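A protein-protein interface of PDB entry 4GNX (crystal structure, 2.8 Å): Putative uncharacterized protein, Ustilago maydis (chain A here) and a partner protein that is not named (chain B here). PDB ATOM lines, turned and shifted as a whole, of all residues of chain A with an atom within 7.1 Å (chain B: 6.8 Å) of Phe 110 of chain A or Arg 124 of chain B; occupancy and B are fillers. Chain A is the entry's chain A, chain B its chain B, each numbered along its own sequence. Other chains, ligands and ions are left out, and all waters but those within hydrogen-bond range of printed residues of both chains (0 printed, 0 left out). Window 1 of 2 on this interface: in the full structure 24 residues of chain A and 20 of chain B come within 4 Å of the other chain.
The backbone carbonyl oxygen (O) of Gly 62 of chain B lies within hydrogen-bond range of the backbone NH (N) of Thr 5 of chain A (2.8 Å).
The guanidinium group (NH1) of Arg 22 of chain A sits close to the backbone NH (N) of Gly 62 of chain B, at 3.3 Å.
OG of Ser 103 of chain A lies within hydrogen-bond range of NH1 of Arg 124 of chain B (3.2 Å).
The backbone carbonyl oxygen (O) of Leu 109 of chain A lies within hydrogen-bond range of the side-chain hydroxyl (OG1) of Thr 13 of chain B, 3.1 Å away.
OD1 of Asp 112 of chain A lies within salt-bridge range of NH1 of Arg 15 of chain B.
The backbone carbonyl oxygen (O) of Asp 61 of chain B is in hydrogen-bond range of the guanidinium group (NH2) of Arg 124 of chain B, at 3.5 Å.
The backbone carbonyl oxygen of Val 99 of chain A sits at hydrogen-bond distance from the side-chain hydroxyl of Ser 103 of chain A, at 2.6 Å.
The side-chain carboxylate (OD1) of Asp 61 of chain B is in hydrogen-bond range of the backbone NH (N) of Thr 63 of chain B (2.8 Å).
OD1 of Asp 61 of chain B sits at hydrogen-bond distance from N of Gly 64 of chain B (3.3 Å).
The guanidinium group (NH1) of Arg 15 of chain B lies within hydrogen-bond range of the backbone carbonyl oxygen (O) of Thr 63 of chain B, at 2.4 Å.
The side-chain hydroxyl (OG1) of Thr 13 of chain B lies close to the backbone NH (N) of Arg 15 of chain B (3.4 Å).
Among the printed residues, merely in contact across the chains: Ser 111 of chain A with Arg 15 of chain B (3.3 Å), Pro 4 of chain A with Gly 62 of chain B (3.4 Å), Leu 109 of chain A with Arg 15 of chain B (3.4 Å), Phe 110 of chain A with Arg 124 of chain B (3.5 Å), Ile 102 of chain A with Leu 125 of chain B (3.6 Å), Phe 110 of chain A with Val 128 of chain B (3.6 Å), Pro 4 of chain A with Arg 15 of chain B (3.7 Å), Phe 106 of chain A with Val 128 of chain B (3.7 Å), Val 99 of chain A with Leu 125 of chain B (3.8 Å), Val 99 of chain A with Arg 124 of chain B (3.8 Å), Arg 22 of chain A with Asp 61 of chain B (3.8 Å), Pro 4 of chain A with Thr 63 of chain B (3.9 Å), Leu 109 of chain A with Ala 127 of chain B (3.9 Å), Phe 110 of chain A with Thr 13 of chain B (3.9 Å), Leu 7 of chain A with Arg 124 of chain B (3.9 Å), Val 99 of chain A with Met 121 of chain B (3.9 Å), Phe 110 of chain A with Thr 63 of chain B (3.9 Å), Leu 109 of chain A with Thr 63 of chain B (3.9 Å) and Leu 7 of chain A with Met 121 of chain B (3.9 Å).
Of the printed residues of chain B, Arg 22 of chain A touches Asp 61 (3.8 Å) and Gly 62 (3.3 Å).
Asn 108 of chain A touches none of the printed residues of chain B.
Phe 110 of chain A touches just these residues of chain B: Thr 13 (3.9 Å), Thr 63 (3.9 Å), Arg 124 (3.5 Å) and Val 128 (3.6 Å).
Of the printed residues of chain A, Thr 13 of chain B touches Leu 109 (3.1 Å) and Phe 110 (3.9 Å).
Of chain A, only Leu 7, Val 99, Ser 103 and Phe 110 come within 4 Å of Arg 124 of chain B.
The nearest residue of chain B that does not touch Phe 110 of chain A is Gly 62 of chain B (4.1 Å).
The nearest residue of chain A that does not touch Arg 124 of chain B is Thr 5 of chain A (5.0 Å).
Of the 18 printed residues of chain B, 10 touch a printed residue of chain A.
Printed residues of chain B that touch a printed residue of chain A: Thr 13, Arg 15, Asp 61, Gly 62, Thr 63, Met 121, Arg 124, Leu 125, Ala 127 and Val 128.
Hydrophobic or aromatic side chains of chain B that line the printed part of chain A: Met 121, Leu 125 and Val 128.
Among the printed residues, 24 pairs touch across the chains.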
ATOM      1  N   PRO A   4      -1.983  22.395   6.549  1.00  0.00           N
ATOM      2  CA  PRO A   4      -1.055  23.106   7.401  1.00  0.00           C
ATOM      3  C   PRO A   4      -1.088  24.588   7.089  1.00  0.00           C
ATOM      4  O   PRO A   4      -1.296  24.965   5.941  1.00  0.00           O
ATOM      5  CB  PRO A   4       0.292  22.498   7.015  1.00  0.00           C
ATOM      6  CG  PRO A   4      -0.054  21.079   6.696  1.00  0.00           C
ATOM      7  CD  PRO A   4      -1.408  21.137   6.035  1.00  0.00           C
ATOM      8  N   THR A   5      -0.908  25.406   8.125  1.00  0.00           N
ATOM      9  CA  THR A   5      -0.806  26.842   7.983  1.00  0.00           C
ATOM     10  C   THR A   5       0.593  27.324   8.382  1.00  0.00           C
ATOM     11  O   THR A   5       0.828  27.613   9.546  1.00  0.00           O
ATOM     12  CB  THR A   5      -1.910  27.530   8.804  1.00  0.00           C
ATOM     13  OG1 THR A   5      -3.153  27.328   8.136  1.00  0.00           O
ATOM     14  CG2 THR A   5      -1.688  29.025   8.898  1.00  0.00           C
ATOM     15  N   PRO A   6       1.531  27.417   7.412  1.00  0.00           N
ATOM     16  CA  PRO A   6       2.901  27.866   7.688  1.00  0.00           C
ATOM     17  C   PRO A   6       3.010  29.080   8.616  1.00  0.00           C
ATOM     18  O   PRO A   6       2.234  30.039   8.485  1.00  0.00           O
ATOM     19  CB  PRO A   6       3.452  28.227   6.285  1.00  0.00           C
ATOM     20  CG  PRO A   6       2.285  28.181   5.368  1.00  0.00           C
ATOM     21  CD  PRO A   6       1.336  27.192   5.970  1.00  0.00           C
ATOM     22  N   LEU A   7       3.982  29.032   9.528  1.00  0.00           N
ATOM     23  CA  LEU A   7       4.371  30.189  10.349  1.00  0.00           C
ATOM     24  C   LEU A   7       5.388  30.924   9.553  1.00  0.00           C
ATOM     25  O   LEU A   7       6.470  30.392   9.303  1.00  0.00           O
ATOM     26  CB  LEU A   7       5.033  29.734  11.646  1.00  0.00           C
ATOM     27  CG  LEU A   7       5.138  30.737  12.782  1.00  0.00           C
ATOM     28  CD1 LEU A   7       3.761  31.195  13.260  1.00  0.00           C
ATOM     29  CD2 LEU A   7       5.942  30.126  13.916  1.00  0.00           C
ATOM     30  N   ARG A  22       0.108  32.067   8.768  1.00  0.00           N
ATOM     31  CA  ARG A  22       0.064  32.499  10.144  1.00  0.00           C
ATOM     32  C   ARG A  22       1.282  33.363  10.362  1.00  0.00           C
ATOM     33  O   ARG A  22       2.372  32.995   9.949  1.00  0.00           O
ATOM     34  CB  ARG A  22       0.109  31.283  11.038  1.00  0.00           C
ATOM     35  CG  ARG A  22      -0.111  31.584  12.501  1.00  0.00           C
ATOM     36  CD  ARG A  22      -0.652  30.345  13.215  1.00  0.00           C
ATOM     37  NE  ARG A  22      -2.076  30.161  12.939  1.00  0.00           N
ATOM     38  CZ  ARG A  22      -2.758  29.065  13.231  1.00  0.00           C
ATOM     39  NH1 ARG A  22      -2.145  28.052  13.811  1.00  0.00           N
ATOM     40  NH2 ARG A  22      -4.052  28.975  12.936  1.00  0.00           N
ATOM     41  N   VAL A  99      12.333  30.071  15.188  1.00  0.00           N
ATOM     42  CA  VAL A  99      11.335  29.050  15.086  1.00  0.00           C
ATOM     43  C   VAL A  99      10.792  29.029  13.668  1.00  0.00           C
ATOM     44  O   VAL A  99      10.556  27.961  13.111  1.00  0.00           O
ATOM     45  CB  VAL A  99      10.248  29.311  16.110  1.00  0.00           C
ATOM     46  CG1 VAL A  99       9.058  28.368  15.914  1.00  0.00           C
ATOM     47  CG2 VAL A  99      10.868  29.160  17.485  1.00  0.00           C
ATOM     48  N   VAL A 100      10.637  30.204  13.059  1.00  0.00           N
ATOM     49  CA  VAL A 100      10.182  30.245  11.669  1.00  0.00           C
ATOM     50  C   VAL A 100      11.149  29.466  10.787  1.00  0.00           C
ATOM     51  O   VAL A 100      10.749  28.506  10.118  1.00  0.00           O
ATOM     52  CB  VAL A 100      10.030  31.663  11.132  1.00  0.00           C
ATOM     53  CG1 VAL A 100       9.981  31.642   9.601  1.00  0.00           C
ATOM     54  CG2 VAL A 100       8.776  32.274  11.709  1.00  0.00           C
ATOM     55  N   ILE A 102      13.453  27.314  11.550  1.00  0.00           N
ATOM     56  CA  ILE A 102      13.606  25.894  11.919  1.00  0.00           C
ATOM     57  C   ILE A 102      12.397  25.090  11.466  1.00  0.00           C
ATOM     58  O   ILE A 102      12.537  23.967  10.961  1.00  0.00           O
ATOM     59  CB  ILE A 102      13.811  25.699  13.433  1.00  0.00           C
ATOM     60  CG1 ILE A 102      15.203  26.160  13.843  1.00  0.00           C
ATOM     61  CG2 ILE A 102      13.736  24.239  13.798  1.00  0.00           C
ATOM     62  CD1 ILE A 102      15.393  26.396  15.331  1.00  0.00           C
ATOM     63  N   SER A 103      11.212  25.671  11.653  1.00  0.00           N
ATOM     64  CA  SER A 103       9.976  25.034  11.204  1.00  0.00           C
ATOM     65  C   SER A 103       9.977  24.829   9.694  1.00  0.00           C
ATOM     66  O   SER A 103       9.501  23.797   9.219  1.00  0.00           O
ATOM     67  CB  SER A 103       8.733  25.820  11.624  1.00  0.00           C
ATOM     68  OG  SER A 103       8.704  26.082  13.028  1.00  0.00           O
ATOM     69  N   ALA A 104      10.523  25.780   8.941  1.00  0.00           N
ATOM     70  CA  ALA A 104      10.647  25.612   7.505  1.00  0.00           C
ATOM     71  C   ALA A 104      11.548  24.416   7.172  1.00  0.00           C
ATOM     72  O   ALA A 104      11.352  23.753   6.154  1.00  0.00           O
ATOM     73  CB  ALA A 104      11.154  26.896   6.870  1.00  0.00           C
ATOM     74  N   ALA A 105      12.512  24.119   8.045  1.00  0.00           N
ATOM     75  CA  ALA A 105      13.469  23.048   7.789  1.00  0.00           C
ATOM     76  C   ALA A 105      13.005  21.691   8.238  1.00  0.00           C
ATOM     77  O   ALA A 105      13.757  20.746   8.135  1.00  0.00           O
ATOM     78  CB  ALA A 105      14.787  23.364   8.456  1.00  0.00           C
ATOM     79  N   PHE A 106      11.797  21.580   8.791  1.00  0.00           N
ATOM     80  CA  PHE A 106      11.286  20.263   9.260  1.00  0.00           C
ATOM     81  C   PHE A 106       9.867  19.981   8.794  1.00  0.00           C
ATOM     82  O   PHE A 106       8.977  19.789   9.613  1.00  0.00           O
ATOM     83  CB  PHE A 106      11.390  20.122  10.776  1.00  0.00           C
ATOM     84  CG  PHE A 106      12.801  20.016  11.274  1.00  0.00           C
ATOM     85  CD1 PHE A 106      13.555  21.157  11.547  1.00  0.00           C
ATOM     86  CD2 PHE A 106      13.389  18.777  11.460  1.00  0.00           C
ATOM     87  CE1 PHE A 106      14.868  21.057  12.007  1.00  0.00           C
ATOM     88  CE2 PHE A 106      14.695  18.666  11.921  1.00  0.00           C
ATOM     89  CZ  PHE A 106      15.433  19.804  12.207  1.00  0.00           C
ATOM     90  N   PRO A 107       9.663  19.938   7.461  1.00  0.00           N
ATOM     91  CA  PRO A 107       8.318  19.822   6.938  1.00  0.00           C
ATOM     92  C   PRO A 107       7.637  18.533   7.394  1.00  0.00           C
ATOM     93  O   PRO A 107       6.409  18.480   7.425  1.00  0.00           O
ATOM     94  CB  PRO A 107       8.533  19.845   5.417  1.00  0.00           C
ATOM     95  CG  PRO A 107       9.923  19.364   5.230  1.00  0.00           C
ATOM     96  CD  PRO A 107      10.661  19.965   6.376  1.00  0.00           C
ATOM     97  N   ASN A 108       8.410  17.514   7.754  1.00  0.00           N
ATOM     98  CA  ASN A 108       7.826  16.277   8.317  1.00  0.00           C
ATOM     99  C   ASN A 108       7.049  16.506   9.628  1.00  0.00           C
ATOM    100  O   ASN A 108       6.136  15.748   9.957  1.00  0.00           O
ATOM    101  CB  ASN A 108       8.888  15.173   8.475  1.00  0.00           C
ATOM    102  CG  ASN A 108      10.203  15.686   9.089  1.00  0.00           C
ATOM    103  OD1 ASN A 108      10.470  16.905   9.128  1.00  0.00           O
ATOM    104  ND2 ASN A 108      11.040  14.750   9.574  1.00  0.00           N
ATOM    105  N   LEU A 109       7.398  17.578  10.340  1.00  0.00           N
ATOM    106  CA  LEU A 109       6.740  17.955  11.590  1.00  0.00           C
ATOM    107  C   LEU A 109       5.723  19.070  11.443  1.00  0.00           C
ATOM    108  O   LEU A 109       4.759  19.106  12.197  1.00  0.00           O
ATOM    109  CB  LEU A 109       7.763  18.418  12.636  1.00  0.00           C
ATOM    110  CG  LEU A 109       8.915  17.561  13.148  1.00  0.00           C
ATOM    111  CD1 LEU A 109       9.003  17.767  14.641  1.00  0.00           C
ATOM    112  CD2 LEU A 109       8.750  16.086  12.868  1.00  0.00           C
ATOM    113  N   PHE A 110       5.948  19.998  10.515  1.00  0.00           N
ATOM    114  CA  PHE A 110       5.102  21.193  10.426  1.00  0.00           C
ATOM    115  C   PHE A 110       4.244  21.293   9.160  1.00  0.00           C
ATOM    116  O   PHE A 110       3.476  22.242   8.982  1.00  0.00           O
ATOM    117  CB  PHE A 110       5.951  22.425  10.628  1.00  0.00           C
ATOM    118  CG  PHE A 110       6.704  22.429  11.939  1.00  0.00           C
ATOM    119  CD1 PHE A 110       8.075  22.157  11.972  1.00  0.00           C
ATOM    120  CD2 PHE A 110       6.045  22.686  13.154  1.00  0.00           C
ATOM    121  CE1 PHE A 110       8.773  22.155  13.180  1.00  0.00           C
ATOM    122  CE2 PHE A 110       6.747  22.672  14.356  1.00  0.00           C
ATOM    123  CZ  PHE A 110       8.106  22.414  14.371  1.00  0.00           C
ATOM    124  N   SER A 111       4.323  20.274   8.304  1.00  0.00           N
ATOM    125  CA  SER A 111       3.661  20.330   7.020  1.00  0.00           C
ATOM    126  C   SER A 111       3.251  18.984   6.478  1.00  0.00           C
ATOM    127  O   SER A 111       3.464  17.970   7.135  1.00  0.00           O
ATOM    128  CB  SER A 111       4.568  21.021   6.030  1.00  0.00           C
ATOM    129  OG  SER A 111       3.760  21.697   5.071  1.00  0.00           O
ATOM    130  N   ASP A 112       2.671  18.981   5.274  1.00  0.00           N
ATOM    131  CA  ASP A 112       2.253  17.753   4.565  1.00  0.00           C
ATOM    132  C   ASP A 112       3.384  16.929   3.960  1.00  0.00           C
ATOM    133  O   ASP A 112       3.366  16.601   2.771  1.00  0.00           O
ATOM    134  CB  ASP A 112       1.259  18.105   3.460  1.00  0.00           C
ATOM    135  CG  ASP A 112      -0.154  18.231   3.977  1.00  0.00           C
ATOM    136  OD1 ASP A 112      -0.420  17.613   5.035  1.00  0.00           O
ATOM    137  OD2 ASP A 112      -0.988  18.931   3.339  1.00  0.00           O
ATOM    138  N   THR B  13       3.870  17.478  17.636  1.00  0.00           N
ATOM    139  CA  THR B  13       2.953  18.319  16.868  1.00  0.00           C
ATOM    140  C   THR B  13       1.773  17.472  16.463  1.00  0.00           C
ATOM    141  O   THR B  13       1.861  16.249  16.373  1.00  0.00           O
ATOM    142  CB  THR B  13       3.577  18.804  15.563  1.00  0.00           C
ATOM    143  OG1 THR B  13       3.821  17.656  14.714  1.00  0.00           O
ATOM    144  CG2 THR B  13       4.873  19.622  15.833  1.00  0.00           C
ATOM    145  N   ARG B  15       0.665  17.084  13.673  1.00  0.00           N
ATOM    146  CA  ARG B  15       1.054  16.322  12.481  1.00  0.00           C
ATOM    147  C   ARG B  15       1.695  14.976  12.797  1.00  0.00           C
ATOM    148  O   ARG B  15       1.373  13.950  12.149  1.00  0.00           O
ATOM    149  CB  ARG B  15       2.024  17.095  11.629  1.00  0.00           C
ATOM    150  CG  ARG B  15       2.163  16.545  10.223  1.00  0.00           C
ATOM    151  CD  ARG B  15       1.163  17.270   9.338  1.00  0.00           C
ATOM    152  NE  ARG B  15       0.021  16.446   8.956  1.00  0.00           N
ATOM    153  CZ  ARG B  15      -1.160  16.907   8.564  1.00  0.00           C
ATOM    154  NH1 ARG B  15      -1.416  18.213   8.520  1.00  0.00           N
ATOM    155  NH2 ARG B  15      -2.102  16.043   8.231  1.00  0.00           N
ATOM    156  N   VAL B  42       0.800  22.185  22.263  1.00  0.00           N
ATOM    157  CA  VAL B  42       0.177  23.490  22.435  1.00  0.00           C
ATOM    158  C   VAL B  42      -0.604  23.768  21.171  1.00  0.00           C
ATOM    159  O   VAL B  42      -0.155  23.446  20.083  1.00  0.00           O
ATOM    160  CB  VAL B  42       1.237  24.566  22.651  1.00  0.00           C
ATOM    161  CG1 VAL B  42       0.606  25.944  22.637  1.00  0.00           C
ATOM    162  CG2 VAL B  42       1.976  24.331  23.965  1.00  0.00           C
ATOM    163  N   ASP B  61      -2.996  23.532  15.637  1.00  0.00           N
ATOM    164  CA  ASP B  61      -1.682  24.155  15.885  1.00  0.00           C
ATOM    165  C   ASP B  61      -0.918  24.490  14.598  1.00  0.00           C
ATOM    166  O   ASP B  61       0.308  24.407  14.558  1.00  0.00           O
ATOM    167  CB  ASP B  61      -0.814  23.207  16.704  1.00  0.00           C
ATOM    168  CG  ASP B  61      -0.353  21.965  15.899  1.00  0.00           C
ATOM    169  OD1 ASP B  61      -0.796  21.800  14.728  1.00  0.00           O
ATOM    170  OD2 ASP B  61       0.453  21.145  16.426  1.00  0.00           O
ATOM    171  N   GLY B  62      -1.631  24.813  13.523  1.00  0.00           N
ATOM    172  CA  GLY B  62      -0.991  25.177  12.278  1.00  0.00           C
ATOM    173  C   GLY B  62      -0.385  24.008  11.528  1.00  0.00           C
ATOM    174  O   GLY B  62       0.102  24.180  10.398  1.00  0.00           O
ATOM    175  N   THR B  63      -0.395  22.821  12.134  1.00  0.00           N
ATOM    176  CA  THR B  63       0.184  21.667  11.460  1.00  0.00           C
ATOM    177  C   THR B  63      -0.849  20.587  11.124  1.00  0.00           C
ATOM    178  O   THR B  63      -0.612  19.722  10.268  1.00  0.00           O
ATOM    179  CB  THR B  63       1.367  21.061  12.247  1.00  0.00           C
ATOM    180  OG1 THR B  63       0.892  20.101  13.214  1.00  0.00           O
ATOM    181  CG2 THR B  63       2.180  22.145  12.920  1.00  0.00           C
ATOM    182  N   GLY B  64      -1.982  20.643  11.818  1.00  0.00           N
ATOM    183  CA  GLY B  64      -3.121  19.743  11.590  1.00  0.00           C
ATOM    184  C   GLY B  64      -4.142  20.017  12.679  1.00  0.00           C
ATOM    185  O   GLY B  64      -3.900  20.868  13.537  1.00  0.00           O
ATOM    186  N   GLU B 119       5.832  30.351  25.113  1.00  0.00           N
ATOM    187  CA  GLU B 119       5.671  28.930  25.326  1.00  0.00           C
ATOM    188  C   GLU B 119       5.307  28.193  24.039  1.00  0.00           C
ATOM    189  O   GLU B 119       5.833  27.095  23.769  1.00  0.00           O
ATOM    190  CB  GLU B 119       4.627  28.647  26.383  1.00  0.00           C
ATOM    191  CG  GLU B 119       4.551  27.161  26.730  1.00  0.00           C
ATOM    192  CD  GLU B 119       3.591  26.841  27.870  1.00  0.00           C
ATOM    193  OE1 GLU B 119       2.754  27.699  28.265  1.00  0.00           O
ATOM    194  OE2 GLU B 119       3.673  25.709  28.379  1.00  0.00           O
ATOM    195  N   VAL B 120       4.406  28.786  23.251  1.00  0.00           N
ATOM    196  CA  VAL B 120       4.038  28.248  21.944  1.00  0.00           C
ATOM    197  C   VAL B 120       5.297  28.040  21.090  1.00  0.00           C
ATOM    198  O   VAL B 120       5.485  26.996  20.440  1.00  0.00           O
ATOM    199  CB  VAL B 120       3.117  29.195  21.195  1.00  0.00           C
ATOM    200  CG1 VAL B 120       2.618  28.523  19.933  1.00  0.00           C
ATOM    201  CG2 VAL B 120       1.942  29.634  22.068  1.00  0.00           C
ATOM    202  N   MET B 121       6.185  29.027  21.122  1.00  0.00           N
ATOM    203  CA  MET B 121       7.420  28.929  20.377  1.00  0.00           C
ATOM    204  C   MET B 121       8.309  27.856  20.958  1.00  0.00           C
ATOM    205  O   MET B 121       8.827  27.022  20.233  1.00  0.00           O
ATOM    206  CB  MET B 121       8.115  30.284  20.324  1.00  0.00           C
ATOM    207  CG  MET B 121       7.242  31.349  19.677  1.00  0.00           C
ATOM    208  SD  MET B 121       6.988  30.996  17.923  1.00  0.00           S
ATOM    209  CE  MET B 121       5.359  30.258  17.817  1.00  0.00           C
ATOM    210  N   PHE B 122       8.477  27.867  22.273  1.00  0.00           N
ATOM    211  CA  PHE B 122       9.292  26.866  22.973  1.00  0.00           C
ATOM    212  C   PHE B 122       8.834  25.476  22.629  1.00  0.00           C
ATOM    213  O   PHE B 122       9.635  24.577  22.400  1.00  0.00           O
ATOM    214  CB  PHE B 122       9.158  27.066  24.475  1.00  0.00           C
ATOM    215  CG  PHE B 122       9.671  25.923  25.289  1.00  0.00           C
ATOM    216  CD1 PHE B 122      11.012  25.883  25.695  1.00  0.00           C
ATOM    217  CD2 PHE B 122       8.822  24.906  25.682  1.00  0.00           C
ATOM    218  CE1 PHE B 122      11.491  24.836  26.462  1.00  0.00           C
ATOM    219  CE2 PHE B 122       9.304  23.864  26.451  1.00  0.00           C
ATOM    220  CZ  PHE B 122      10.636  23.829  26.835  1.00  0.00           C
ATOM    221  N   HIS B 123       7.524  25.302  22.573  1.00  0.00           N
ATOM    222  CA  HIS B 123       6.999  23.991  22.247  1.00  0.00           C
ATOM    223  C   HIS B 123       7.352  23.408  20.875  1.00  0.00           C
ATOM    224  O   HIS B 123       7.563  22.188  20.761  1.00  0.00           O
ATOM    225  CB  HIS B 123       5.506  23.919  22.443  1.00  0.00           C
ATOM    226  CG  HIS B 123       4.971  22.614  22.023  1.00  0.00           C
ATOM    227  ND1 HIS B 123       5.384  21.465  22.606  1.00  0.00           N
ATOM    228  CD2 HIS B 123       4.134  22.258  20.984  1.00  0.00           C
ATOM    229  CE1 HIS B 123       4.785  20.416  22.001  1.00  0.00           C
ATOM    230  NE2 HIS B 123       4.018  20.898  21.013  1.00  0.00           N
ATOM    231  N   ARG B 124       7.376  24.237  19.823  1.00  0.00           N
ATOM    232  CA  ARG B 124       7.743  23.726  18.514  1.00  0.00           C
ATOM    233  C   ARG B 124       9.166  23.192  18.547  1.00  0.00           C
ATOM    234  O   ARG B 124       9.471  22.126  17.977  1.00  0.00           O
ATOM    235  CB  ARG B 124       7.639  24.805  17.463  1.00  0.00           C
ATOM    236  CG  ARG B 124       6.216  25.119  17.058  1.00  0.00           C
ATOM    237  CD  ARG B 124       6.175  25.843  15.738  1.00  0.00           C
ATOM    238  NE  ARG B 124       4.859  25.668  15.129  1.00  0.00           N
ATOM    239  CZ  ARG B 124       4.588  25.812  13.834  1.00  0.00           C
ATOM    240  NH1 ARG B 124       5.547  26.131  12.975  1.00  0.00           N
ATOM    241  NH2 ARG B 124       3.346  25.626  13.406  1.00  0.00           N
ATOM    242  N   LEU B 125      10.030  23.919  19.251  1.00  0.00           N
ATOM    243  CA  LEU B 125      11.437  23.560  19.341  1.00  0.00           C
ATOM    244  C   LEU B 125      11.615  22.290  20.136  1.00  0.00           C
ATOM    245  O   LEU B 125      12.526  21.502  19.887  1.00  0.00           O
ATOM    246  CB  LEU B 125      12.252  24.697  19.944  1.00  0.00           C
ATOM    247  CG  LEU B 125      12.252  25.997  19.127  1.00  0.00           C
ATOM    248  CD1 LEU B 125      13.036  27.094  19.826  1.00  0.00           C
ATOM    249  CD2 LEU B 125      12.803  25.783  17.724  1.00  0.00           C
ATOM    250  N   GLU B 126      10.737  22.079  21.100  1.00  0.00           N
ATOM    251  CA  GLU B 126      10.894  20.944  21.969  1.00  0.00           C
ATOM    252  C   GLU B 126      10.573  19.697  21.172  1.00  0.00           C
ATOM    253  O   GLU B 126      11.252  18.681  21.306  1.00  0.00           O
ATOM    254  CB  GLU B 126       9.991  21.093  23.183  1.00  0.00           C
ATOM    255  CG  GLU B 126      10.570  20.455  24.438  1.00  0.00           C
ATOM    256  CD  GLU B 126       9.632  20.486  25.639  1.00  0.00           C
ATOM    257  OE1 GLU B 126      10.129  20.095  26.734  1.00  0.00           O
ATOM    258  OE2 GLU B 126       8.427  20.886  25.488  1.00  0.00           O
ATOM    259  N   ALA B 127       9.565  19.803  20.302  1.00  0.00           N
ATOM    260  CA  ALA B 127       9.186  18.717  19.386  1.00  0.00           C
ATOM    261  C   ALA B 127      10.283  18.420  18.400  1.00  0.00           C
ATOM    262  O   ALA B 127      10.581  17.260  18.133  1.00  0.00           O
ATOM    263  CB  ALA B 127       7.918  19.052  18.637  1.00  0.00           C
ATOM    264  N   VAL B 128      10.888  19.464  17.849  1.00  0.00           N
ATOM    265  CA  VAL B 128      12.028  19.264  16.949  1.00  0.00           C
ATOM    266  C   VAL B 128      13.119  18.541  17.739  1.00  0.00           C
ATOM    267  O   VAL B 128      13.571  17.433  17.367  1.00  0.00           O
ATOM    268  CB  VAL B 128      12.525  20.595  16.327  1.00  0.00           C
ATOM    269  CG1 VAL B 128      13.774  20.392  15.495  1.00  0.00           C
ATOM    270  CG2 VAL B 128      11.435  21.197  15.450  1.00  0.00           C
ATOM    271  N   HIS B 129      13.516  19.142  18.851  1.00  0.00           N
ATOM    272  CA  HIS B 129      14.594  18.579  19.652  1.00  0.00           C
ATOM    273  C   HIS B 129      14.339  17.148  20.029  1.00  0.00           C
ATOM    274  O   HIS B 129      15.215  16.297  19.883  1.00  0.00           O
ATOM    275  CB  HIS B 129      14.866  19.439  20.888  1.00  0.00           C
ATOM    276  CG  HIS B 129      16.049  18.978  21.678  1.00  0.00           C
ATOM    277  ND1 HIS B 129      17.308  19.131  21.242  1.00  0.00           N
ATOM    278  CD2 HIS B 129      16.128  18.297  22.874  1.00  0.00           C
ATOM    279  CE1 HIS B 129      18.163  18.590  22.121  1.00  0.00           C
ATOM    280  NE2 HIS B 129      17.443  18.071  23.117  1.00  0.00           N
